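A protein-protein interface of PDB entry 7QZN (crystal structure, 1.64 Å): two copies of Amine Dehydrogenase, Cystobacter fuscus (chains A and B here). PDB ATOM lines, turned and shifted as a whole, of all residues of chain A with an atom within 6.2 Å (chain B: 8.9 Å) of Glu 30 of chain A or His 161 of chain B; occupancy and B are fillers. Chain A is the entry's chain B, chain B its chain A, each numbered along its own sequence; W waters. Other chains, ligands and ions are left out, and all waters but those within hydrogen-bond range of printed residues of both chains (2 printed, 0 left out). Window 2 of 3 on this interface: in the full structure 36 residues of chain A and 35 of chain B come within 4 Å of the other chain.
CE1 of His 161 of chain B touches O of Thr 27 of chain A (3.3 Å). Lys 31 of chain A touches Thr 160 of chain B. OE2 of Glu 293 of chain B touches CB of Ala 307 of chain A (3.6 Å). Ala 159 of chain B touches Ala 311 of chain A. His 161 of chain B touches Ala 311 of chain A. Ala 157 of chain B touches Tyr 338 of chain A (O to CB, 3.5 Å). N of Tyr 338 of chain A touches CA of Gly 158 of chain B, at 3.9 Å. O of Thr 160 of chain B touches CD1 of Tyr 338 of chain A, at 3.5 Å. O of His 161 of chain B touches CE1 of Tyr 338 of chain A, 3.5 Å away. Tyr 338 of chain A touches Arg 162 of chain B.
Water W1 lies within hydrogen-bond range of OE1 of Glu 30 of chain A (2.7 Å) and NE2 of His 161 of chain B (3.5 Å). Water W2 lies within hydrogen-bond range of O of His 161 of chain B (3.2 Å) and OH of Tyr 338 of chain A (3.5 Å).
The backbone carbonyl oxygen (O) of Gly 158 of chain B sits at hydrogen-bond distance from the side-chain amide nitrogen (ND2) of Asn 315 of chain A (2.9 Å). The backbone carbonyl oxygen (O) of Thr 160 of chain B is in hydrogen-bond range of the side-chain amide nitrogen (ND2) of Asn 315 of chain A, at 3.0 Å. NE2 of His 161 of chain B sits at hydrogen-bond distance from OE1 of Glu 30 of chain A, at 2.8 Å. O of His 161 of chain B sits close to NZ of Lys 31 of chain A, 2.9 Å away. The backbone NH (N) of Ile 163 of chain B is in hydrogen-bond range of the side-chain hydroxyl (OH) of Tyr 338 of chain A (3.0 Å).
Printed residues of chain A that touch a printed residue of chain B: Thr 27, Glu 30, Lys 31, Ala 307, Ala 311, Asn 315 and Tyr 338. Hydrophobic or aromatic side chains of chain A within 4 Å of the printed part of chain B: Ala 307, Ala 311 and Tyr 338. Of the 16 printed residues of chain B, 9 touch a printed residue of chain A. Hydrophobic or aromatic side chains of chain B within 4 Å of the printed part of chain A: Ala 157, His 161, Ile 163 and Pro 294. Among the printed residues, 18 pairs touch across the chains. Among the printed residues, no Asp or Glu carboxylate lies within 4 Å of a Lys or Arg side-chain nitrogen of the other chain.
Thr 27 of chain A touches just one residue of chain B: His 161. Of chain B, only His 161 (2.8 Å) comes within 4 Å of Glu 30 of chain A. Lys 31 of chain A touches two residues of chain B. Ala 33 of chain A touches none of the printed residues of chain B. Of the printed residues of chain B, Ala 307 of chain A touches Glu 293 (3.6 Å) and Pro 294 (3.9 Å). Printed residues of chain B within 4 Å of Asn 315 of chain A: Ala 157, Gly 158 and Thr 160. Printed residues of chain A within 4 Å of Ala 157 of chain B: Asn 315 (3.7 Å) and Tyr 338 (3.5 Å). Of chain A, only Thr 27 (3.3 Å), Glu 30 (2.8 Å), Lys 31 (2.8 Å), Ala 311 (3.4 Å) and Tyr 338 (3.5 Å) come within 4 Å of His 161 of chain B. Printed residues of chain A within 4 Å of Glu 293 of chain B: Ala 307. Of the printed residues of chain A, Pro 294 of chain B touches Ala 307.
No position is printed for both chains.
The backbone carbonyl oxygen of Leu 156 of chain B lies within hydrogen-bond range of the side-chain hydroxyl of Thr 160 of chain B, 3.1 Å away. N of His 161 of chain B lies within hydrogen-bond range of O of Glu 293 of chain B. The backbone carbonyl oxygen (O) of Arg 162 of chain B lies within hydrogen-bond range of the backbone NH (N) of Glu 293 of chain B (2.8 Å). NZ of Lys 31 of chain A is in hydrogen-bond range of OD1 of Asn 315 of chain A, at 2.9 Å. O of Val 339 of chain A sits at hydrogen-bond distance from NZ of Lys 31 of chain A, 2.8 Å away. The side-chain amide oxygen of Asn 315 of chain A lies within hydrogen-bond range of the backbone NH of Val 339 of chain A (3.0 Å).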
ATOM      1  N   ILE A  25      -0.715  13.816  -6.209  1.00  0.00           N
ATOM      2  CA  ILE A  25      -2.181  13.534  -6.243  1.00  0.00           C
ATOM      3  C   ILE A  25      -2.468  12.538  -7.375  1.00  0.00           C
ATOM      4  O   ILE A  25      -3.270  11.632  -7.196  1.00  0.00           O
ATOM      5  CB  ILE A  25      -2.978  14.845  -6.386  1.00  0.00           C
ATOM      6  CG1 ILE A  25      -3.009  15.636  -5.078  1.00  0.00           C
ATOM      7  CG2 ILE A  25      -4.376  14.582  -6.921  1.00  0.00           C
ATOM      8  CD1 ILE A  25      -3.218  17.119  -5.267  1.00  0.00           C
ATOM      9  N   ARG A  26      -1.809  12.723  -8.499  1.00  0.00           N
ATOM     10  CA  ARG A  26      -1.989  11.813  -9.647  1.00  0.00           C
ATOM     11  C   ARG A  26      -1.371  10.451  -9.347  1.00  0.00           C
ATOM     12  O   ARG A  26      -2.040   9.443  -9.560  1.00  0.00           O
ATOM     13  CB  ARG A  26      -1.261  12.449 -10.832  1.00  0.00           C
ATOM     14  CG  ARG A  26      -1.635  11.911 -12.200  1.00  0.00           C
ATOM     15  CD  ARG A  26      -1.010  12.801 -13.256  1.00  0.00           C
ATOM     16  NE  ARG A  26      -0.758  14.169 -12.834  1.00  0.00           N
ATOM     17  CZ  ARG A  26       0.446  14.710 -12.708  1.00  0.00           C
ATOM     18  NH1 ARG A  26       1.527  13.988 -12.949  1.00  0.00           N
ATOM     19  NH2 ARG A  26       0.567  15.967 -12.327  1.00  0.00           N
ATOM     20  N   THR A  27      -0.128  10.439  -8.864  1.00  0.00           N
ATOM     21  CA  THR A  27       0.606   9.160  -8.673  1.00  0.00           C
ATOM     22  C   THR A  27       0.003   8.325  -7.549  1.00  0.00           C
ATOM     23  O   THR A  27       0.026   7.110  -7.658  1.00  0.00           O
ATOM     24  CB  THR A  27       2.107   9.436  -8.469  1.00  0.00           C
ATOM     25  OG1 THR A  27       2.321  10.465  -7.506  1.00  0.00           O
ATOM     26  CG2 THR A  27       2.781   9.827  -9.766  1.00  0.00           C
ATOM     27  N   LEU A  28      -0.487   8.977  -6.499  1.00  0.00           N
ATOM     28  CA  LEU A  28      -0.982   8.194  -5.346  1.00  0.00           C
ATOM     29  C   LEU A  28      -2.188   7.359  -5.799  1.00  0.00           C
ATOM     30  O   LEU A  28      -2.325   6.231  -5.344  1.00  0.00           O
ATOM     31  CB  LEU A  28      -1.299   9.116  -4.156  1.00  0.00           C
ATOM     32  CG  LEU A  28      -2.499  10.052  -4.273  1.00  0.00           C
ATOM     33  CD1 LEU A  28      -3.772   9.362  -3.808  1.00  0.00           C
ATOM     34  CD2 LEU A  28      -2.258  11.305  -3.445  1.00  0.00           C
ATOM     35  N   ARG A  29      -2.978   7.910  -6.699  1.00  0.00           N
ATOM     36  CA  ARG A  29      -4.165   7.189  -7.205  1.00  0.00           C
ATOM     37  C   ARG A  29      -3.743   6.026  -8.104  1.00  0.00           C
ATOM     38  O   ARG A  29      -4.376   4.982  -8.047  1.00  0.00           O
ATOM     39  CB  ARG A  29      -5.032   8.180  -7.972  1.00  0.00           C
ATOM     40  CG  ARG A  29      -5.492   9.349  -7.115  1.00  0.00           C
ATOM     41  CD  ARG A  29      -6.474  10.259  -7.818  1.00  0.00           C
ATOM     42  NE  ARG A  29      -7.715   9.571  -8.123  1.00  0.00           N
ATOM     43  CZ  ARG A  29      -8.073   9.167  -9.336  1.00  0.00           C
ATOM     44  NH1 ARG A  29      -7.276   9.373 -10.369  1.00  0.00           N
ATOM     45  NH2 ARG A  29      -9.226   8.550  -9.507  1.00  0.00           N
ATOM     46  N   GLU A  30      -2.709   6.241  -8.912  1.00  0.00           N
ATOM     47  CA  GLU A  30      -2.219   5.167  -9.804  1.00  0.00           C
ATOM     48  C   GLU A  30      -1.740   3.972  -8.967  1.00  0.00           C
ATOM     49  O   GLU A  30      -1.716   2.875  -9.503  1.00  0.00           O
ATOM     50  CB  GLU A  30      -1.137   5.708 -10.744  1.00  0.00           C
ATOM     51  CG  GLU A  30      -1.592   6.836 -11.649  1.00  0.00           C
ATOM     52  CD  GLU A  30      -0.498   7.447 -12.511  1.00  0.00           C
ATOM     53  OE1 GLU A  30       0.642   6.975 -12.437  1.00  0.00           O
ATOM     54  OE2 GLU A  30      -0.791   8.398 -13.249  1.00  0.00           O
ATOM     55  N   LYS A  31      -1.386   4.185  -7.704  1.00  0.00           N
ATOM     56  CA  LYS A  31      -0.872   3.084  -6.855  1.00  0.00           C
ATOM     57  C   LYS A  31      -1.976   2.604  -5.912  1.00  0.00           C
ATOM     58  O   LYS A  31      -1.674   1.840  -5.007  1.00  0.00           O
ATOM     59  CB  LYS A  31       0.372   3.507  -6.077  1.00  0.00           C
ATOM     60  CG  LYS A  31       1.585   3.854  -6.921  1.00  0.00           C
ATOM     61  CD  LYS A  31       2.866   3.519  -6.217  1.00  0.00           C
ATOM     62  CE  LYS A  31       3.882   2.921  -7.158  1.00  0.00           C
ATOM     63  NZ  LYS A  31       5.244   2.944  -6.580  1.00  0.00           N
ATOM     64  N   GLY A  32      -3.193   3.082  -6.106  1.00  0.00           N
ATOM     65  CA  GLY A  32      -4.310   2.538  -5.315  1.00  0.00           C
ATOM     66  C   GLY A  32      -4.665   3.289  -4.053  1.00  0.00           C
ATOM     67  O   GLY A  32      -5.509   2.781  -3.313  1.00  0.00           O
ATOM     68  N   ALA A  33      -4.058   4.450  -3.811  1.00  0.00           N
ATOM     69  CA  ALA A  33      -4.454   5.262  -2.644  1.00  0.00           C
ATOM     70  C   ALA A  33      -5.578   6.226  -3.027  1.00  0.00           C
ATOM     71  O   ALA A  33      -5.820   6.409  -4.214  1.00  0.00           O
ATOM     72  CB  ALA A  33      -3.266   6.003  -2.092  1.00  0.00           C
ATOM     73  N   ALA A 307      10.401  13.494  -9.980  1.00  0.00           N
ATOM     74  CA  ALA A 307       9.679  12.206 -10.045  1.00  0.00           C
ATOM     75  C   ALA A 307      10.222  11.237  -8.983  1.00  0.00           C
ATOM     76  O   ALA A 307       9.403  10.567  -8.306  1.00  0.00           O
ATOM     77  CB  ALA A 307       9.737  11.619 -11.435  1.00  0.00           C
ATOM     78  N   ALA A 311       8.017   9.642  -5.929  1.00  0.00           N
ATOM     79  CA  ALA A 311       7.869   8.172  -5.922  1.00  0.00           C
ATOM     80  C   ALA A 311       8.408   7.579  -4.605  1.00  0.00           C
ATOM     81  O   ALA A 311       7.814   6.653  -4.060  1.00  0.00           O
ATOM     82  CB  ALA A 311       8.538   7.620  -7.126  1.00  0.00           C
ATOM     83  N   LEU A 314       5.804   8.015  -1.816  1.00  0.00           N
ATOM     84  CA  LEU A 314       4.655   7.069  -1.863  1.00  0.00           C
ATOM     85  C   LEU A 314       5.133   5.671  -1.499  1.00  0.00           C
ATOM     86  O   LEU A 314       4.445   4.991  -0.746  1.00  0.00           O
ATOM     87  CB  LEU A 314       3.999   7.094  -3.237  1.00  0.00           C
ATOM     88  CG  LEU A 314       3.358   8.432  -3.614  1.00  0.00           C
ATOM     89  CD1 LEU A 314       2.681   8.334  -4.956  1.00  0.00           C
ATOM     90  CD2 LEU A 314       2.375   8.883  -2.546  1.00  0.00           C
ATOM     91  N   ASN A 315       6.317   5.259  -1.956  1.00  0.00           N
ATOM     92  CA  ASN A 315       6.842   3.917  -1.608  1.00  0.00           C
ATOM     93  C   ASN A 315       7.053   3.780  -0.088  1.00  0.00           C
ATOM     94  O   ASN A 315       6.960   2.655   0.408  1.00  0.00           O
ATOM     95  CB  ASN A 315       8.102   3.563  -2.394  1.00  0.00           C
ATOM     96  CG  ASN A 315       7.788   3.228  -3.837  1.00  0.00           C
ATOM     97  OD1 ASN A 315       6.748   2.660  -4.157  1.00  0.00           O
ATOM     98  ND2 ASN A 315       8.692   3.587  -4.729  1.00  0.00           N
ATOM     99  N   TYR A 338       9.872  -0.859  -3.630  1.00  0.00           N
ATOM    100  CA  TYR A 338       8.860  -0.598  -4.662  1.00  0.00           C
ATOM    101  C   TYR A 338       7.508  -1.184  -4.232  1.00  0.00           C
ATOM    102  O   TYR A 338       7.420  -2.406  -3.941  1.00  0.00           O
ATOM    103  CB  TYR A 338       9.339  -1.232  -5.960  1.00  0.00           C
ATOM    104  CG  TYR A 338       8.386  -1.055  -7.104  1.00  0.00           C
ATOM    105  CD1 TYR A 338       8.235   0.175  -7.722  1.00  0.00           C
ATOM    106  CD2 TYR A 338       7.675  -2.141  -7.606  1.00  0.00           C
ATOM    107  CE1 TYR A 338       7.423   0.332  -8.827  1.00  0.00           C
ATOM    108  CE2 TYR A 338       6.839  -1.989  -8.701  1.00  0.00           C
ATOM    109  CZ  TYR A 338       6.707  -0.760  -9.313  1.00  0.00           C
ATOM    110  OH  TYR A 338       5.879  -0.589 -10.386  1.00  0.00           O
ATOM    111  N   VAL A 339       6.479  -0.349  -4.228  1.00  0.00           N
ATOM    112  CA  VAL A 339       5.106  -0.723  -3.784  1.00  0.00           C
ATOM    113  C   VAL A 339       4.205  -0.552  -5.008  1.00  0.00           C
ATOM    114  O   VAL A 339       4.224   0.532  -5.607  1.00  0.00           O
ATOM    115  CB  VAL A 339       4.698   0.143  -2.576  1.00  0.00           C
ATOM    116  CG1 VAL A 339       3.284  -0.136  -2.099  1.00  0.00           C
ATOM    117  CG2 VAL A 339       5.671  -0.084  -1.430  1.00  0.00           C
ATOM    118  N   SER A 340       3.518  -1.626  -5.412  1.00  0.00           N
ATOM    119  CA  SER A 340       2.548  -1.587  -6.533  1.00  0.00           C
ATOM    120  C   SER A 340       1.234  -1.010  -6.021  1.00  0.00           C
ATOM    121  O   SER A 340       0.560  -0.344  -6.802  1.00  0.00           O
ATOM    122  CB  SER A 340       2.332  -2.961  -7.135  1.00  0.00           C
ATOM    123  OG  SER A 340       3.132  -3.100  -8.288  1.00  0.00           O
ATOM    124  N   LEU B 156      17.151   1.470  -5.713  1.00  0.00           N
ATOM    125  CA  LEU B 156      16.646   2.398  -6.733  1.00  0.00           C
ATOM    126  C   LEU B 156      15.162   2.158  -7.032  1.00  0.00           C
ATOM    127  O   LEU B 156      14.435   3.160  -7.255  1.00  0.00           O
ATOM    128  CB  LEU B 156      17.533   2.306  -7.975  1.00  0.00           C
ATOM    129  CG  LEU B 156      18.971   2.754  -7.740  1.00  0.00           C
ATOM    130  CD1 LEU B 156      19.879   2.315  -8.868  1.00  0.00           C
ATOM    131  CD2 LEU B 156      19.052   4.269  -7.542  1.00  0.00           C
ATOM    132  N   ALA B 157      14.717   0.900  -7.009  1.00  0.00           N
ATOM    133  CA  ALA B 157      13.293   0.570  -7.221  1.00  0.00           C
ATOM    134  C   ALA B 157      12.440   1.265  -6.154  1.00  0.00           C
ATOM    135  O   ALA B 157      11.307   1.664  -6.463  1.00  0.00           O
ATOM    136  CB  ALA B 157      13.097  -0.916  -7.250  1.00  0.00           C
ATOM    137  N   GLY B 158      12.988   1.494  -4.961  1.00  0.00           N
ATOM    138  CA  GLY B 158      12.305   2.201  -3.851  1.00  0.00           C
ATOM    139  C   GLY B 158      12.028   3.666  -4.178  1.00  0.00           C
ATOM    140  O   GLY B 158      11.186   4.247  -3.495  1.00  0.00           O
ATOM    141  N   ALA B 159      12.670   4.252  -5.201  1.00  0.00           N
ATOM    142  CA  ALA B 159      12.469   5.652  -5.638  1.00  0.00           C
ATOM    143  C   ALA B 159      11.688   5.716  -6.950  1.00  0.00           C
ATOM    144  O   ALA B 159      11.587   6.789  -7.525  1.00  0.00           O
ATOM    145  CB  ALA B 159      13.802   6.358  -5.760  1.00  0.00           C
ATOM    146  N   THR B 160      11.085   4.604  -7.387  1.00  0.00           N
ATOM    147  CA  THR B 160      10.498   4.473  -8.742  1.00  0.00           C
ATOM    148  C   THR B 160       8.987   4.400  -8.634  1.00  0.00           C
ATOM    149  O   THR B 160       8.489   3.694  -7.729  1.00  0.00           O
ATOM    150  CB  THR B 160      11.064   3.280  -9.504  1.00  0.00           C
ATOM    151  OG1 THR B 160      12.492   3.430  -9.601  1.00  0.00           O
ATOM    152  CG2 THR B 160      10.473   3.195 -10.905  1.00  0.00           C
ATOM    153  N   HIS B 161       8.278   5.153  -9.464  1.00  0.00           N
ATOM    154  CA  HIS B 161       6.790   5.127  -9.442  1.00  0.00           C
ATOM    155  C   HIS B 161       6.257   3.851 -10.085  1.00  0.00           C
ATOM    156  O   HIS B 161       5.448   3.120  -9.481  1.00  0.00           O
ATOM    157  CB  HIS B 161       6.219   6.325 -10.156  1.00  0.00           C
ATOM    158  CG  HIS B 161       4.729   6.287 -10.170  1.00  0.00           C
ATOM    159  ND1 HIS B 161       3.997   6.157  -9.010  1.00  0.00           N
ATOM    160  CD2 HIS B 161       3.856   6.264 -11.203  1.00  0.00           C
ATOM    161  CE1 HIS B 161       2.720   6.085  -9.347  1.00  0.00           C
ATOM    162  NE2 HIS B 161       2.618   6.192 -10.668  1.00  0.00           N
ATOM    163  N   ARG B 162       6.712   3.591 -11.293  1.00  0.00           N
ATOM    164  CA  ARG B 162       6.226   2.399 -12.029  1.00  0.00           C
ATOM    165  C   ARG B 162       7.446   1.772 -12.701  1.00  0.00           C
ATOM    166  O   ARG B 162       8.177   2.510 -13.389  1.00  0.00           O
ATOM    167  CB  ARG B 162       5.180   2.772 -13.084  1.00  0.00           C
ATOM    168  CG  ARG B 162       4.509   1.556 -13.701  1.00  0.00           C
ATOM    169  CD  ARG B 162       3.633   1.876 -14.915  1.00  0.00           C
ATOM    170  NE  ARG B 162       4.456   2.263 -16.043  1.00  0.00           N
ATOM    171  CZ  ARG B 162       4.620   3.480 -16.524  1.00  0.00           C
ATOM    172  NH1 ARG B 162       3.918   4.497 -16.054  1.00  0.00           N
ATOM    173  NH2 ARG B 162       5.480   3.685 -17.508  1.00  0.00           N
ATOM    174  N   ILE B 163       7.640   0.461 -12.516  1.00  0.00           N
ATOM    175  CA  ILE B 163       8.712  -0.259 -13.254  1.00  0.00           C
ATOM    176  C   ILE B 163       8.075  -1.088 -14.368  1.00  0.00           C
ATOM    177  O   ILE B 163       7.235  -1.938 -14.085  1.00  0.00           O
ATOM    178  CB  ILE B 163       9.524  -1.150 -12.320  1.00  0.00           C
ATOM    179  CG1 ILE B 163      10.229  -0.328 -11.237  1.00  0.00           C
ATOM    180  CG2 ILE B 163      10.464  -1.984 -13.124  1.00  0.00           C
ATOM    181  CD1 ILE B 163      10.712  -1.172 -10.074  1.00  0.00           C
ATOM    182  N   ASP B 164       8.490  -0.814 -15.591  1.00  0.00           N
ATOM    183  CA  ASP B 164       8.071  -1.600 -16.780  1.00  0.00           C
ATOM    184  C   ASP B 164       9.133  -2.668 -17.030  1.00  0.00           C
ATOM    185  O   ASP B 164       8.800  -3.800 -17.352  1.00  0.00           O
ATOM    186  CB  ASP B 164       7.907  -0.673 -17.965  1.00  0.00           C
ATOM    187  CG  ASP B 164       6.767   0.324 -17.843  1.00  0.00           C
ATOM    188  OD1 ASP B 164       5.811   0.063 -17.038  1.00  0.00           O
ATOM    189  OD2 ASP B 164       6.872   1.365 -18.510  1.00  0.00           O
ATOM    190  N   LEU B 290      16.285   1.254 -14.718  1.00  0.00           N
ATOM    191  CA  LEU B 290      14.873   1.003 -14.392  1.00  0.00           C
ATOM    192  C   LEU B 290      14.046   1.830 -15.374  1.00  0.00           C
ATOM    193  O   LEU B 290      14.102   3.036 -15.314  1.00  0.00           O
ATOM    194  CB  LEU B 290      14.634   1.348 -12.919  1.00  0.00           C
ATOM    195  CG  LEU B 290      15.321   0.438 -11.914  1.00  0.00           C
ATOM    196  CD1 LEU B 290      16.718   0.947 -11.601  1.00  0.00           C
ATOM    197  CD2 LEU B 290      14.530   0.346 -10.619  1.00  0.00           C
ATOM    198  N   ARG B 291      13.410   1.159 -16.335  1.00  0.00           N
ATOM    199  CA  ARG B 291      12.552   1.798 -17.369  1.00  0.00           C
ATOM    200  C   ARG B 291      11.119   1.832 -16.853  1.00  0.00           C
ATOM    201  O   ARG B 291      10.579   0.791 -16.428  1.00  0.00           O
ATOM    202  CB  ARG B 291      12.672   1.027 -18.680  1.00  0.00           C
ATOM    203  CG  ARG B 291      14.038   1.146 -19.339  1.00  0.00           C
ATOM    204  CD  ARG B 291      14.067   0.601 -20.756  1.00  0.00           C
ATOM    205  NE  ARG B 291      15.413   0.383 -21.297  1.00  0.00           N
ATOM    206  CZ  ARG B 291      15.697  -0.473 -22.269  1.00  0.00           C
ATOM    207  NH1 ARG B 291      14.727  -1.212 -22.796  1.00  0.00           N
ATOM    208  NH2 ARG B 291      16.946  -0.614 -22.705  1.00  0.00           N
ATOM    209  N   GLY B 292      10.499   3.001 -16.901  1.00  0.00           N
ATOM    210  CA  GLY B 292       9.106   3.183 -16.454  1.00  0.00           C
ATOM    211  C   GLY B 292       8.910   4.627 -16.086  1.00  0.00           C
ATOM    212  O   GLY B 292       9.276   5.488 -16.879  1.00  0.00           O
ATOM    213  N   GLU B 293       8.390   4.892 -14.903  1.00  0.00           N
ATOM    214  CA  GLU B 293       8.209   6.290 -14.485  1.00  0.00           C
ATOM    215  C   GLU B 293       8.918   6.469 -13.160  1.00  0.00           C
ATOM    216  O   GLU B 293       8.545   5.832 -12.180  1.00  0.00           O
ATOM    217  CB  GLU B 293       6.729   6.627 -14.287  1.00  0.00           C
ATOM    218  CG  GLU B 293       6.514   8.077 -13.803  1.00  0.00           C
ATOM    219  CD  GLU B 293       7.291   9.101 -14.608  1.00  0.00           C
ATOM    220  OE1 GLU B 293       7.434   8.882 -15.861  1.00  0.00           O
ATOM    221  OE2 GLU B 293       7.790  10.098 -14.020  1.00  0.00           O
ATOM    222  N   PRO B 294       9.976   7.290 -13.082  1.00  0.00           N
ATOM    223  CA  PRO B 294      10.745   7.780 -14.207  1.00  0.00           C
ATOM    224  C   PRO B 294      11.702   6.659 -14.669  1.00  0.00           C
ATOM    225  O   PRO B 294      11.800   5.606 -14.033  1.00  0.00           O
ATOM    226  CB  PRO B 294      11.540   8.927 -13.566  1.00  0.00           C
ATOM    227  CG  PRO B 294      11.857   8.397 -12.184  1.00  0.00           C
ATOM    228  CD  PRO B 294      10.642   7.585 -11.809  1.00  0.00           C
ATOM    229  N   ASP B 295      12.444   6.920 -15.745  1.00  0.00           N
ATOM    230  CA  ASP B 295      13.616   6.110 -16.141  1.00  0.00           C
ATOM    231  C   ASP B 295      14.793   6.547 -15.276  1.00  0.00           C
ATOM    232  O   ASP B 295      15.035   7.783 -15.135  1.00  0.00           O
ATOM    233  CB  ASP B 295      13.966   6.304 -17.612  1.00  0.00           C
ATOM    234  CG  ASP B 295      13.014   5.669 -18.616  1.00  0.00           C
ATOM    235  OD1 ASP B 295      12.104   4.943 -18.267  1.00  0.00           O
ATOM    236  OD2 ASP B 295      13.268   5.895 -19.792  1.00  0.00           O
ATOM    237  N   THR B 296      15.470   5.586 -14.667  1.00  0.00           N
ATOM    238  CA  THR B 296      16.697   5.849 -13.887  1.00  0.00           C
ATOM    239  C   THR B 296      17.827   4.965 -14.369  1.00  0.00           C
ATOM    240  O   THR B 296      17.629   3.740 -14.495  1.00  0.00           O
ATOM    241  CB  THR B 296      16.470   5.652 -12.378  1.00  0.00           C
ATOM    242  OG1 THR B 296      15.435   6.539 -11.946  1.00  0.00           O
ATOM    243  CG2 THR B 296      17.737   5.918 -11.612  1.00  0.00           C
HETATM  244  O   HOH W   1       2.762   8.150 -13.550  1.00  0.00           O
HETATM  245  O   HOH W   2       2.956   1.306 -10.267  1.00  0.00           O
